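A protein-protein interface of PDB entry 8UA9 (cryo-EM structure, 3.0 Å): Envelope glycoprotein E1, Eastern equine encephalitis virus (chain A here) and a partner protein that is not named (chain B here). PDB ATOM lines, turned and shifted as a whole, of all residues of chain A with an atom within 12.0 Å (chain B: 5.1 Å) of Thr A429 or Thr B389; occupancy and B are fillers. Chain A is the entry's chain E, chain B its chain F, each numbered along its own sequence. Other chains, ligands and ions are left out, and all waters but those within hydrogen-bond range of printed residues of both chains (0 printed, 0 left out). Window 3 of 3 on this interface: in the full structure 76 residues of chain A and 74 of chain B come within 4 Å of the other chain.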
ATOM      1  N   ALA A 420     -23.066  -0.531  -9.239  1.00  0.00           N
ATOM      2  CA  ALA A 420     -21.975  -0.231  -8.331  1.00  0.00           C
ATOM      3  C   ALA A 420     -22.273  -0.736  -6.937  1.00  0.00           C
ATOM      4  O   ALA A 420     -21.383  -1.262  -6.269  1.00  0.00           O
ATOM      5  CB  ALA A 420     -21.710   1.273  -8.308  1.00  0.00           C
ATOM      6  N   PHE A 421     -23.506  -0.576  -6.469  1.00  0.00           N
ATOM      7  CA  PHE A 421     -23.826  -1.069  -5.141  1.00  0.00           C
ATOM      8  C   PHE A 421     -23.685  -2.582  -5.065  1.00  0.00           C
ATOM      9  O   PHE A 421     -23.105  -3.115  -4.111  1.00  0.00           O
ATOM     10  CB  PHE A 421     -25.228  -0.641  -4.736  1.00  0.00           C
ATOM     11  CG  PHE A 421     -25.307  -0.068  -3.357  1.00  0.00           C
ATOM     12  CD1 PHE A 421     -24.709  -0.700  -2.286  1.00  0.00           C
ATOM     13  CD2 PHE A 421     -26.007   1.095  -3.128  1.00  0.00           C
ATOM     14  CE1 PHE A 421     -24.791  -0.174  -1.018  1.00  0.00           C
ATOM     15  CE2 PHE A 421     -26.097   1.628  -1.861  1.00  0.00           C
ATOM     16  CZ  PHE A 421     -25.488   0.992  -0.804  1.00  0.00           C
ATOM     17  N   ILE A 422     -24.165  -3.292  -6.085  1.00  0.00           N
ATOM     18  CA  ILE A 422     -24.097  -4.749  -6.059  1.00  0.00           C
ATOM     19  C   ILE A 422     -22.657  -5.210  -6.176  1.00  0.00           C
ATOM     20  O   ILE A 422     -22.238  -6.160  -5.511  1.00  0.00           O
ATOM     21  CB  ILE A 422     -24.969  -5.349  -7.179  1.00  0.00           C
ATOM     22  CG1 ILE A 422     -26.481  -5.132  -6.950  1.00  0.00           C
ATOM     23  CG2 ILE A 422     -24.645  -6.847  -7.375  1.00  0.00           C
ATOM     24  CD1 ILE A 422     -26.965  -5.057  -5.533  1.00  0.00           C
ATOM     25  N   VAL A 423     -21.866  -4.538  -7.000  1.00  0.00           N
ATOM     26  CA  VAL A 423     -20.496  -4.973  -7.162  1.00  0.00           C
ATOM     27  C   VAL A 423     -19.707  -4.637  -5.920  1.00  0.00           C
ATOM     28  O   VAL A 423     -18.787  -5.369  -5.547  1.00  0.00           O
ATOM     29  CB  VAL A 423     -19.875  -4.327  -8.413  1.00  0.00           C
ATOM     30  CG1 VAL A 423     -18.362  -4.497  -8.422  1.00  0.00           C
ATOM     31  CG2 VAL A 423     -20.478  -4.929  -9.669  1.00  0.00           C
ATOM     32  N   LEU A 424     -20.040  -3.541  -5.252  1.00  0.00           N
ATOM     33  CA  LEU A 424     -19.393  -3.245  -3.987  1.00  0.00           C
ATOM     34  C   LEU A 424     -19.708  -4.319  -2.969  1.00  0.00           C
ATOM     35  O   LEU A 424     -18.824  -4.756  -2.226  1.00  0.00           O
ATOM     36  CB  LEU A 424     -19.841  -1.879  -3.485  1.00  0.00           C
ATOM     37  CG  LEU A 424     -19.184  -1.234  -2.264  1.00  0.00           C
ATOM     38  CD1 LEU A 424     -19.916  -1.602  -0.982  1.00  0.00           C
ATOM     39  CD2 LEU A 424     -17.702  -1.568  -2.139  1.00  0.00           C
ATOM     40  N   GLY A 425     -20.951  -4.779  -2.936  1.00  0.00           N
ATOM     41  CA  GLY A 425     -21.274  -5.880  -2.050  1.00  0.00           C
ATOM     42  C   GLY A 425     -20.493  -7.140  -2.371  1.00  0.00           C
ATOM     43  O   GLY A 425     -19.959  -7.791  -1.476  1.00  0.00           O
ATOM     44  N   LEU A 426     -20.374  -7.475  -3.651  1.00  0.00           N
ATOM     45  CA  LEU A 426     -19.698  -8.715  -3.994  1.00  0.00           C
ATOM     46  C   LEU A 426     -18.214  -8.625  -3.694  1.00  0.00           C
ATOM     47  O   LEU A 426     -17.607  -9.594  -3.211  1.00  0.00           O
ATOM     48  CB  LEU A 426     -19.931  -9.061  -5.457  1.00  0.00           C
ATOM     49  CG  LEU A 426     -21.357  -9.298  -5.961  1.00  0.00           C
ATOM     50  CD1 LEU A 426     -21.320 -10.181  -7.201  1.00  0.00           C
ATOM     51  CD2 LEU A 426     -22.264  -9.907  -4.919  1.00  0.00           C
ATOM     52  N   ILE A 427     -17.614  -7.462  -3.924  1.00  0.00           N
ATOM     53  CA  ILE A 427     -16.211  -7.319  -3.582  1.00  0.00           C
ATOM     54  C   ILE A 427     -16.031  -7.330  -2.072  1.00  0.00           C
ATOM     55  O   ILE A 427     -15.014  -7.818  -1.567  1.00  0.00           O
ATOM     56  CB  ILE A 427     -15.642  -6.042  -4.214  1.00  0.00           C
ATOM     57  CG1 ILE A 427     -15.630  -6.129  -5.751  1.00  0.00           C
ATOM     58  CG2 ILE A 427     -14.244  -5.760  -3.676  1.00  0.00           C
ATOM     59  CD1 ILE A 427     -14.864  -7.305  -6.357  1.00  0.00           C
ATOM     60  N   ALA A 428     -17.013  -6.837  -1.318  1.00  0.00           N
ATOM     61  CA  ALA A 428     -16.932  -6.943   0.131  1.00  0.00           C
ATOM     62  C   ALA A 428     -16.980  -8.391   0.581  1.00  0.00           C
ATOM     63  O   ALA A 428     -16.255  -8.787   1.505  1.00  0.00           O
ATOM     64  CB  ALA A 428     -18.065  -6.154   0.780  1.00  0.00           C
ATOM     65  N   THR A 429     -17.840  -9.194  -0.042  1.00  0.00           N
ATOM     66  CA  THR A 429     -17.908 -10.601   0.333  1.00  0.00           C
ATOM     67  C   THR A 429     -16.586 -11.283   0.048  1.00  0.00           C
ATOM     68  O   THR A 429     -16.097 -12.084   0.859  1.00  0.00           O
ATOM     69  CB  THR A 429     -19.054 -11.311  -0.376  1.00  0.00           C
ATOM     70  OG1 THR A 429     -20.259 -11.051   0.338  1.00  0.00           O
ATOM     71  CG2 THR A 429     -18.860 -12.843  -0.455  1.00  0.00           C
ATOM     72  N   ALA A 430     -15.991 -10.993  -1.097  1.00  0.00           N
ATOM     73  CA  ALA A 430     -14.698 -11.596  -1.360  1.00  0.00           C
ATOM     74  C   ALA A 430     -13.657 -11.138  -0.347  1.00  0.00           C
ATOM     75  O   ALA A 430     -12.820 -11.938   0.089  1.00  0.00           O
ATOM     76  CB  ALA A 430     -14.238 -11.263  -2.775  1.00  0.00           C
ATOM     77  N   VAL A 431     -13.678  -9.861   0.038  1.00  0.00           N
ATOM     78  CA  VAL A 431     -12.653  -9.393   0.962  1.00  0.00           C
ATOM     79  C   VAL A 431     -12.794 -10.063   2.319  1.00  0.00           C
ATOM     80  O   VAL A 431     -11.791 -10.416   2.952  1.00  0.00           O
ATOM     81  CB  VAL A 431     -12.703  -7.862   1.080  1.00  0.00           C
ATOM     82  CG1 VAL A 431     -11.910  -7.373   2.290  1.00  0.00           C
ATOM     83  CG2 VAL A 431     -12.164  -7.224  -0.180  1.00  0.00           C
ATOM     84  N   VAL A 432     -14.025 -10.282   2.780  1.00  0.00           N
ATOM     85  CA  VAL A 432     -14.189 -10.983   4.051  1.00  0.00           C
ATOM     86  C   VAL A 432     -13.701 -12.412   3.944  1.00  0.00           C
ATOM     87  O   VAL A 432     -13.090 -12.941   4.881  1.00  0.00           O
ATOM     88  CB  VAL A 432     -15.609 -10.890   4.618  1.00  0.00           C
ATOM     89  CG1 VAL A 432     -15.890  -9.457   4.926  1.00  0.00           C
ATOM     90  CG2 VAL A 432     -16.642 -11.437   3.677  1.00  0.00           C
ATOM     91  N   ALA A 433     -14.019 -13.088   2.846  1.00  0.00           N
ATOM     92  CA  ALA A 433     -13.559 -14.459   2.737  1.00  0.00           C
ATOM     93  C   ALA A 433     -12.046 -14.506   2.777  1.00  0.00           C
ATOM     94  O   ALA A 433     -11.457 -15.342   3.474  1.00  0.00           O
ATOM     95  CB  ALA A 433     -14.081 -15.090   1.450  1.00  0.00           C
ATOM     96  N   LEU A 434     -11.398 -13.593   2.072  1.00  0.00           N
ATOM     97  CA  LEU A 434      -9.948 -13.622   2.045  1.00  0.00           C
ATOM     98  C   LEU A 434      -9.354 -13.295   3.402  1.00  0.00           C
ATOM     99  O   LEU A 434      -8.367 -13.919   3.811  1.00  0.00           O
ATOM    100  CB  LEU A 434      -9.435 -12.656   0.985  1.00  0.00           C
ATOM    101  CG  LEU A 434      -7.970 -12.768   0.561  1.00  0.00           C
ATOM    102  CD1 LEU A 434      -7.853 -12.950  -0.945  1.00  0.00           C
ATOM    103  CD2 LEU A 434      -7.190 -11.531   0.999  1.00  0.00           C
ATOM    104  N   VAL A 435      -9.929 -12.339   4.127  1.00  0.00           N
ATOM    105  CA  VAL A 435      -9.328 -12.000   5.411  1.00  0.00           C
ATOM    106  C   VAL A 435      -9.519 -13.131   6.401  1.00  0.00           C
ATOM    107  O   VAL A 435      -8.644 -13.391   7.226  1.00  0.00           O
ATOM    108  CB  VAL A 435      -9.834 -10.663   5.982  1.00  0.00           C
ATOM    109  CG1 VAL A 435      -9.480  -9.507   5.051  1.00  0.00           C
ATOM    110  CG2 VAL A 435     -11.286 -10.723   6.322  1.00  0.00           C
ATOM    111  N   LEU A 436     -10.647 -13.833   6.343  1.00  0.00           N
ATOM    112  CA  LEU A 436     -10.800 -14.963   7.246  1.00  0.00           C
ATOM    113  C   LEU A 436      -9.819 -16.079   6.907  1.00  0.00           C
ATOM    114  O   LEU A 436      -9.219 -16.691   7.805  1.00  0.00           O
ATOM    115  CB  LEU A 436     -12.231 -15.465   7.196  1.00  0.00           C
ATOM    116  CG  LEU A 436     -13.251 -14.550   7.860  1.00  0.00           C
ATOM    117  CD1 LEU A 436     -14.645 -15.059   7.588  1.00  0.00           C
ATOM    118  CD2 LEU A 436     -13.030 -14.435   9.353  1.00  0.00           C
ATOM    119  N   PHE A 437      -9.627 -16.345   5.623  1.00  0.00           N
ATOM    120  CA  PHE A 437      -8.670 -17.370   5.241  1.00  0.00           C
ATOM    121  C   PHE A 437      -7.274 -17.013   5.715  1.00  0.00           C
ATOM    122  O   PHE A 437      -6.544 -17.877   6.214  1.00  0.00           O
ATOM    123  CB  PHE A 437      -8.712 -17.520   3.723  1.00  0.00           C
ATOM    124  CG  PHE A 437      -7.869 -18.620   3.165  1.00  0.00           C
ATOM    125  CD1 PHE A 437      -6.509 -18.483   3.014  1.00  0.00           C
ATOM    126  CD2 PHE A 437      -8.462 -19.778   2.730  1.00  0.00           C
ATOM    127  CE1 PHE A 437      -5.757 -19.491   2.481  1.00  0.00           C
ATOM    128  CE2 PHE A 437      -7.718 -20.790   2.193  1.00  0.00           C
ATOM    129  CZ  PHE A 437      -6.360 -20.649   2.067  1.00  0.00           C
ATOM    130  N   PHE A 438      -6.886 -15.754   5.587  1.00  0.00           N
ATOM    131  CA  PHE A 438      -5.626 -15.317   6.168  1.00  0.00           C
ATOM    132  C   PHE A 438      -5.640 -15.330   7.684  1.00  0.00           C
ATOM    133  O   PHE A 438      -4.572 -15.428   8.290  1.00  0.00           O
ATOM    134  CB  PHE A 438      -5.221 -13.944   5.637  1.00  0.00           C
ATOM    135  CG  PHE A 438      -4.658 -13.959   4.228  1.00  0.00           C
ATOM    136  CD1 PHE A 438      -4.033 -15.074   3.686  1.00  0.00           C
ATOM    137  CD2 PHE A 438      -4.749 -12.821   3.452  1.00  0.00           C
ATOM    138  CE1 PHE A 438      -3.532 -15.055   2.412  1.00  0.00           C
ATOM    139  CE2 PHE A 438      -4.241 -12.796   2.167  1.00  0.00           C
ATOM    140  CZ  PHE A 438      -3.632 -13.915   1.647  1.00  0.00           C
ATOM    141  N   HIS A 439      -6.800 -15.230   8.317  1.00  0.00           N
ATOM    142  CA  HIS A 439      -6.824 -15.274   9.770  1.00  0.00           C
ATOM    143  C   HIS A 439      -6.391 -16.643  10.240  1.00  0.00           C
ATOM    144  O   HIS A 439      -5.478 -16.763  11.061  1.00  0.00           O
ATOM    145  CB  HIS A 439      -8.206 -14.972  10.333  1.00  0.00           C
ATOM    146  CG  HIS A 439      -8.510 -13.523  10.487  1.00  0.00           C
ATOM    147  ND1 HIS A 439      -7.548 -12.542  10.429  1.00  0.00           N
ATOM    148  CD2 HIS A 439      -9.682 -12.889  10.711  1.00  0.00           C
ATOM    149  CE1 HIS A 439      -8.115 -11.365  10.606  1.00  0.00           C
ATOM    150  NE2 HIS A 439      -9.410 -11.547  10.778  1.00  0.00           N
ATOM    151  N   TRP B 384     -28.229  -6.047   2.585  1.00  0.00           N
ATOM    152  CA  TRP B 384     -28.156  -7.301   3.319  1.00  0.00           C
ATOM    153  C   TRP B 384     -26.772  -7.895   3.194  1.00  0.00           C
ATOM    154  O   TRP B 384     -26.219  -8.437   4.157  1.00  0.00           O
ATOM    155  CB  TRP B 384     -29.222  -8.252   2.784  1.00  0.00           C
ATOM    156  CG  TRP B 384     -29.020  -9.697   3.054  1.00  0.00           C
ATOM    157  CD1 TRP B 384     -29.592 -10.418   4.044  1.00  0.00           C
ATOM    158  CD2 TRP B 384     -28.219 -10.614   2.299  1.00  0.00           C
ATOM    159  NE1 TRP B 384     -29.191 -11.726   3.970  1.00  0.00           N
ATOM    160  CE2 TRP B 384     -28.344 -11.868   2.906  1.00  0.00           C
ATOM    161  CE3 TRP B 384     -27.399 -10.488   1.181  1.00  0.00           C
ATOM    162  CZ2 TRP B 384     -27.683 -12.989   2.432  1.00  0.00           C
ATOM    163  CZ3 TRP B 384     -26.746 -11.597   0.714  1.00  0.00           C
ATOM    164  CH2 TRP B 384     -26.890 -12.831   1.335  1.00  0.00           C
ATOM    165  N   LEU B 385     -26.181  -7.751   2.028  1.00  0.00           N
ATOM    166  CA  LEU B 385     -24.837  -8.235   1.807  1.00  0.00           C
ATOM    167  C   LEU B 385     -23.838  -7.445   2.630  1.00  0.00           C
ATOM    168  O   LEU B 385     -22.886  -8.014   3.171  1.00  0.00           O
ATOM    169  CB  LEU B 385     -24.525  -8.141   0.324  1.00  0.00           C
ATOM    170  CG  LEU B 385     -23.577  -9.176  -0.236  1.00  0.00           C
ATOM    171  CD1 LEU B 385     -23.758  -9.308  -1.734  1.00  0.00           C
ATOM    172  CD2 LEU B 385     -22.172  -8.816   0.096  1.00  0.00           C
ATOM    173  N   LEU B 386     -24.034  -6.136   2.741  1.00  0.00           N
ATOM    174  CA  LEU B 386     -23.125  -5.333   3.543  1.00  0.00           C
ATOM    175  C   LEU B 386     -23.312  -5.614   5.023  1.00  0.00           C
ATOM    176  O   LEU B 386     -22.345  -5.612   5.788  1.00  0.00           O
ATOM    177  CB  LEU B 386     -23.331  -3.854   3.244  1.00  0.00           C
ATOM    178  CG  LEU B 386     -22.323  -3.185   2.304  1.00  0.00           C
ATOM    179  CD1 LEU B 386     -20.923  -3.118   2.894  1.00  0.00           C
ATOM    180  CD2 LEU B 386     -22.298  -3.885   0.955  1.00  0.00           C
ATOM    181  N   CYS B 387     -24.528  -5.913   5.446  1.00  0.00           N
ATOM    182  CA  CYS B 387     -24.712  -6.304   6.831  1.00  0.00           C
ATOM    183  C   CYS B 387     -23.996  -7.614   7.109  1.00  0.00           C
ATOM    184  O   CYS B 387     -23.316  -7.759   8.132  1.00  0.00           O
ATOM    185  CB  CYS B 387     -26.200  -6.419   7.161  1.00  0.00           C
ATOM    186  SG  CYS B 387     -26.902  -4.957   7.947  1.00  0.00           S
ATOM    187  N   ARG B 388     -24.113  -8.565   6.191  1.00  0.00           N
ATOM    188  CA  ARG B 388     -23.486  -9.864   6.379  1.00  0.00           C
ATOM    189  C   ARG B 388     -21.978  -9.745   6.397  1.00  0.00           C
ATOM    190  O   ARG B 388     -21.301 -10.363   7.231  1.00  0.00           O
ATOM    191  CB  ARG B 388     -23.916 -10.801   5.260  1.00  0.00           C
ATOM    192  CG  ARG B 388     -24.219 -12.194   5.704  1.00  0.00           C
ATOM    193  CD  ARG B 388     -23.956 -13.199   4.620  1.00  0.00           C
ATOM    194  NE  ARG B 388     -22.546 -13.273   4.263  1.00  0.00           N
ATOM    195  CZ  ARG B 388     -21.930 -14.353   3.800  1.00  0.00           C
ATOM    196  NH1 ARG B 388     -22.563 -15.505   3.634  1.00  0.00           N
ATOM    197  NH2 ARG B 388     -20.647 -14.273   3.471  1.00  0.00           N
ATOM    198  N   THR B 389     -21.431  -8.950   5.487  1.00  0.00           N
ATOM    199  CA  THR B 389     -19.991  -8.808   5.421  1.00  0.00           C
ATOM    200  C   THR B 389     -19.489  -8.106   6.674  1.00  0.00           C
ATOM    201  O   THR B 389     -18.411  -8.435   7.183  1.00  0.00           O
ATOM    202  CB  THR B 389     -19.613  -8.081   4.122  1.00  0.00           C
ATOM    203  OG1 THR B 389     -18.288  -8.423   3.732  1.00  0.00           O
ATOM    204  CG2 THR B 389     -19.635  -6.564   4.248  1.00  0.00           C
ATOM    205  N   ARG B 390     -20.300  -7.223   7.255  1.00  0.00           N
ATOM    206  CA  ARG B 390     -19.911  -6.613   8.517  1.00  0.00           C
ATOM    207  C   ARG B 390     -19.923  -7.632   9.640  1.00  0.00           C
ATOM    208  O   ARG B 390     -19.041  -7.621  10.502  1.00  0.00           O
ATOM    209  CB  ARG B 390     -20.849  -5.459   8.865  1.00  0.00           C
ATOM    210  CG  ARG B 390     -20.757  -5.004  10.317  1.00  0.00           C
ATOM    211  CD  ARG B 390     -20.858  -3.512  10.471  1.00  0.00           C
ATOM    212  NE  ARG B 390     -21.099  -3.132  11.856  1.00  0.00           N
ATOM    213  CZ  ARG B 390     -22.199  -3.415  12.541  1.00  0.00           C
ATOM    214  NH1 ARG B 390     -23.254  -3.970  11.966  1.00  0.00           N
ATOM    215  NH2 ARG B 390     -22.251  -3.120  13.836  1.00  0.00           N
ATOM    216  N   ASN B 391     -20.967  -8.449   9.709  1.00  0.00           N
ATOM    217  CA  ASN B 391     -21.049  -9.440  10.773  1.00  0.00           C
ATOM    218  C   ASN B 391     -19.830 -10.330  10.742  1.00  0.00           C
ATOM    219  O   ASN B 391     -19.212 -10.595  11.774  1.00  0.00           O
ATOM    220  CB  ASN B 391     -22.313 -10.268  10.649  1.00  0.00           C
ATOM    221  CG  ASN B 391     -23.319  -9.913  11.688  1.00  0.00           C
ATOM    222  OD1 ASN B 391     -23.517  -8.741  11.991  1.00  0.00           O
ATOM    223  ND2 ASN B 391     -23.963 -10.919  12.262  1.00  0.00           N
ATOM    224  N   LEU B 392     -19.447 -10.769   9.558  1.00  0.00           N
ATOM    225  CA  LEU B 392     -18.248 -11.581   9.448  1.00  0.00           C
ATOM    226  C   LEU B 392     -17.008 -10.792   9.838  1.00  0.00           C
ATOM    227  O   LEU B 392     -16.080 -11.352  10.427  1.00  0.00           O
ATOM    228  CB  LEU B 392     -18.114 -12.134   8.035  1.00  0.00           C
ATOM    229  CG  LEU B 392     -18.937 -13.377   7.681  1.00  0.00           C
ATOM    230  CD1 LEU B 392     -20.305 -13.438   8.352  1.00  0.00           C
ATOM    231  CD2 LEU B 392     -19.102 -13.459   6.174  1.00  0.00           C
ATOM    232  N   CYS B 393     -16.948  -9.506   9.507  1.00  0.00           N
ATOM    233  CA  CYS B 393     -15.766  -8.730   9.880  1.00  0.00           C
ATOM    234  C   CYS B 393     -15.629  -8.600  11.387  1.00  0.00           C
ATOM    235  O   CYS B 393     -14.547  -8.801  11.942  1.00  0.00           O
ATOM    236  CB  CYS B 393     -15.853  -7.322   9.286  1.00  0.00           C
ATOM    237  SG  CYS B 393     -14.858  -6.945   7.842  1.00  0.00           S
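O of Ala A428 is in hydrogen-bond range of OG1 of Thr B389 (3.0 Å).
Of the 20 printed residues of chain A, 6 touch a printed residue of chain B.
Hydrophobic or aromatic side chains of chain B that line the printed part of chain A: Leu B385 and Leu B386.
Among the printed residues, 9 pairs touch across the chains.
Among the printed residues, no Asp or Glu carboxylate lies within 4 Å of a Lys or Arg side-chain nitrogen of the other chain.
Of chain A, only Ala A428 (3.0 Å), Thr A429 (3.9 Å) and Val A432 (2.9 Å) come within 4 Å of Thr B389.
No residue of chain A comes within 4 Å of Cys B387.
No residue of chain A comes within 4 Å of Arg B388.
No residue of chain A comes within 4 Å of Asn B391.
No residue of chain A comes within 4 Å of Leu B392.
Printed residues of chain B within 4 Å of Gly A425: Leu B385 (2.9 Å) and Leu B386 (3.7 Å).
Of the printed residues of chain B, Ala A428 touches Thr B389 (3.0 Å).
Printed residues of chain B within 4 Å of Leu A424: Leu B386.
The nearest residue of chain B that does not touch Thr A429 is Arg B388 (4.5 Å).
The nearest residue of chain A that does not touch Thr B389 is Gly A425 (5.5 Å).
The nearest printed residue of chain A that does not touch Cys B393 is Val A435 (5.4 Å).
Among the printed residues, merely in contact across the chains: Val A432 with Thr B389 (2.9 Å), Gly A425 with Leu B385 (2.9 Å), Thr A429 with Leu B385 (3.0 Å), Leu A426 with Leu B385 (3.6 Å), Gly A425 with Leu B386 (3.7 Å), Leu A424 with Leu B386 (3.8 Å), Thr A429 with Thr B389 (3.9 Å) and Val A432 with Cys B393 (3.98 Å).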
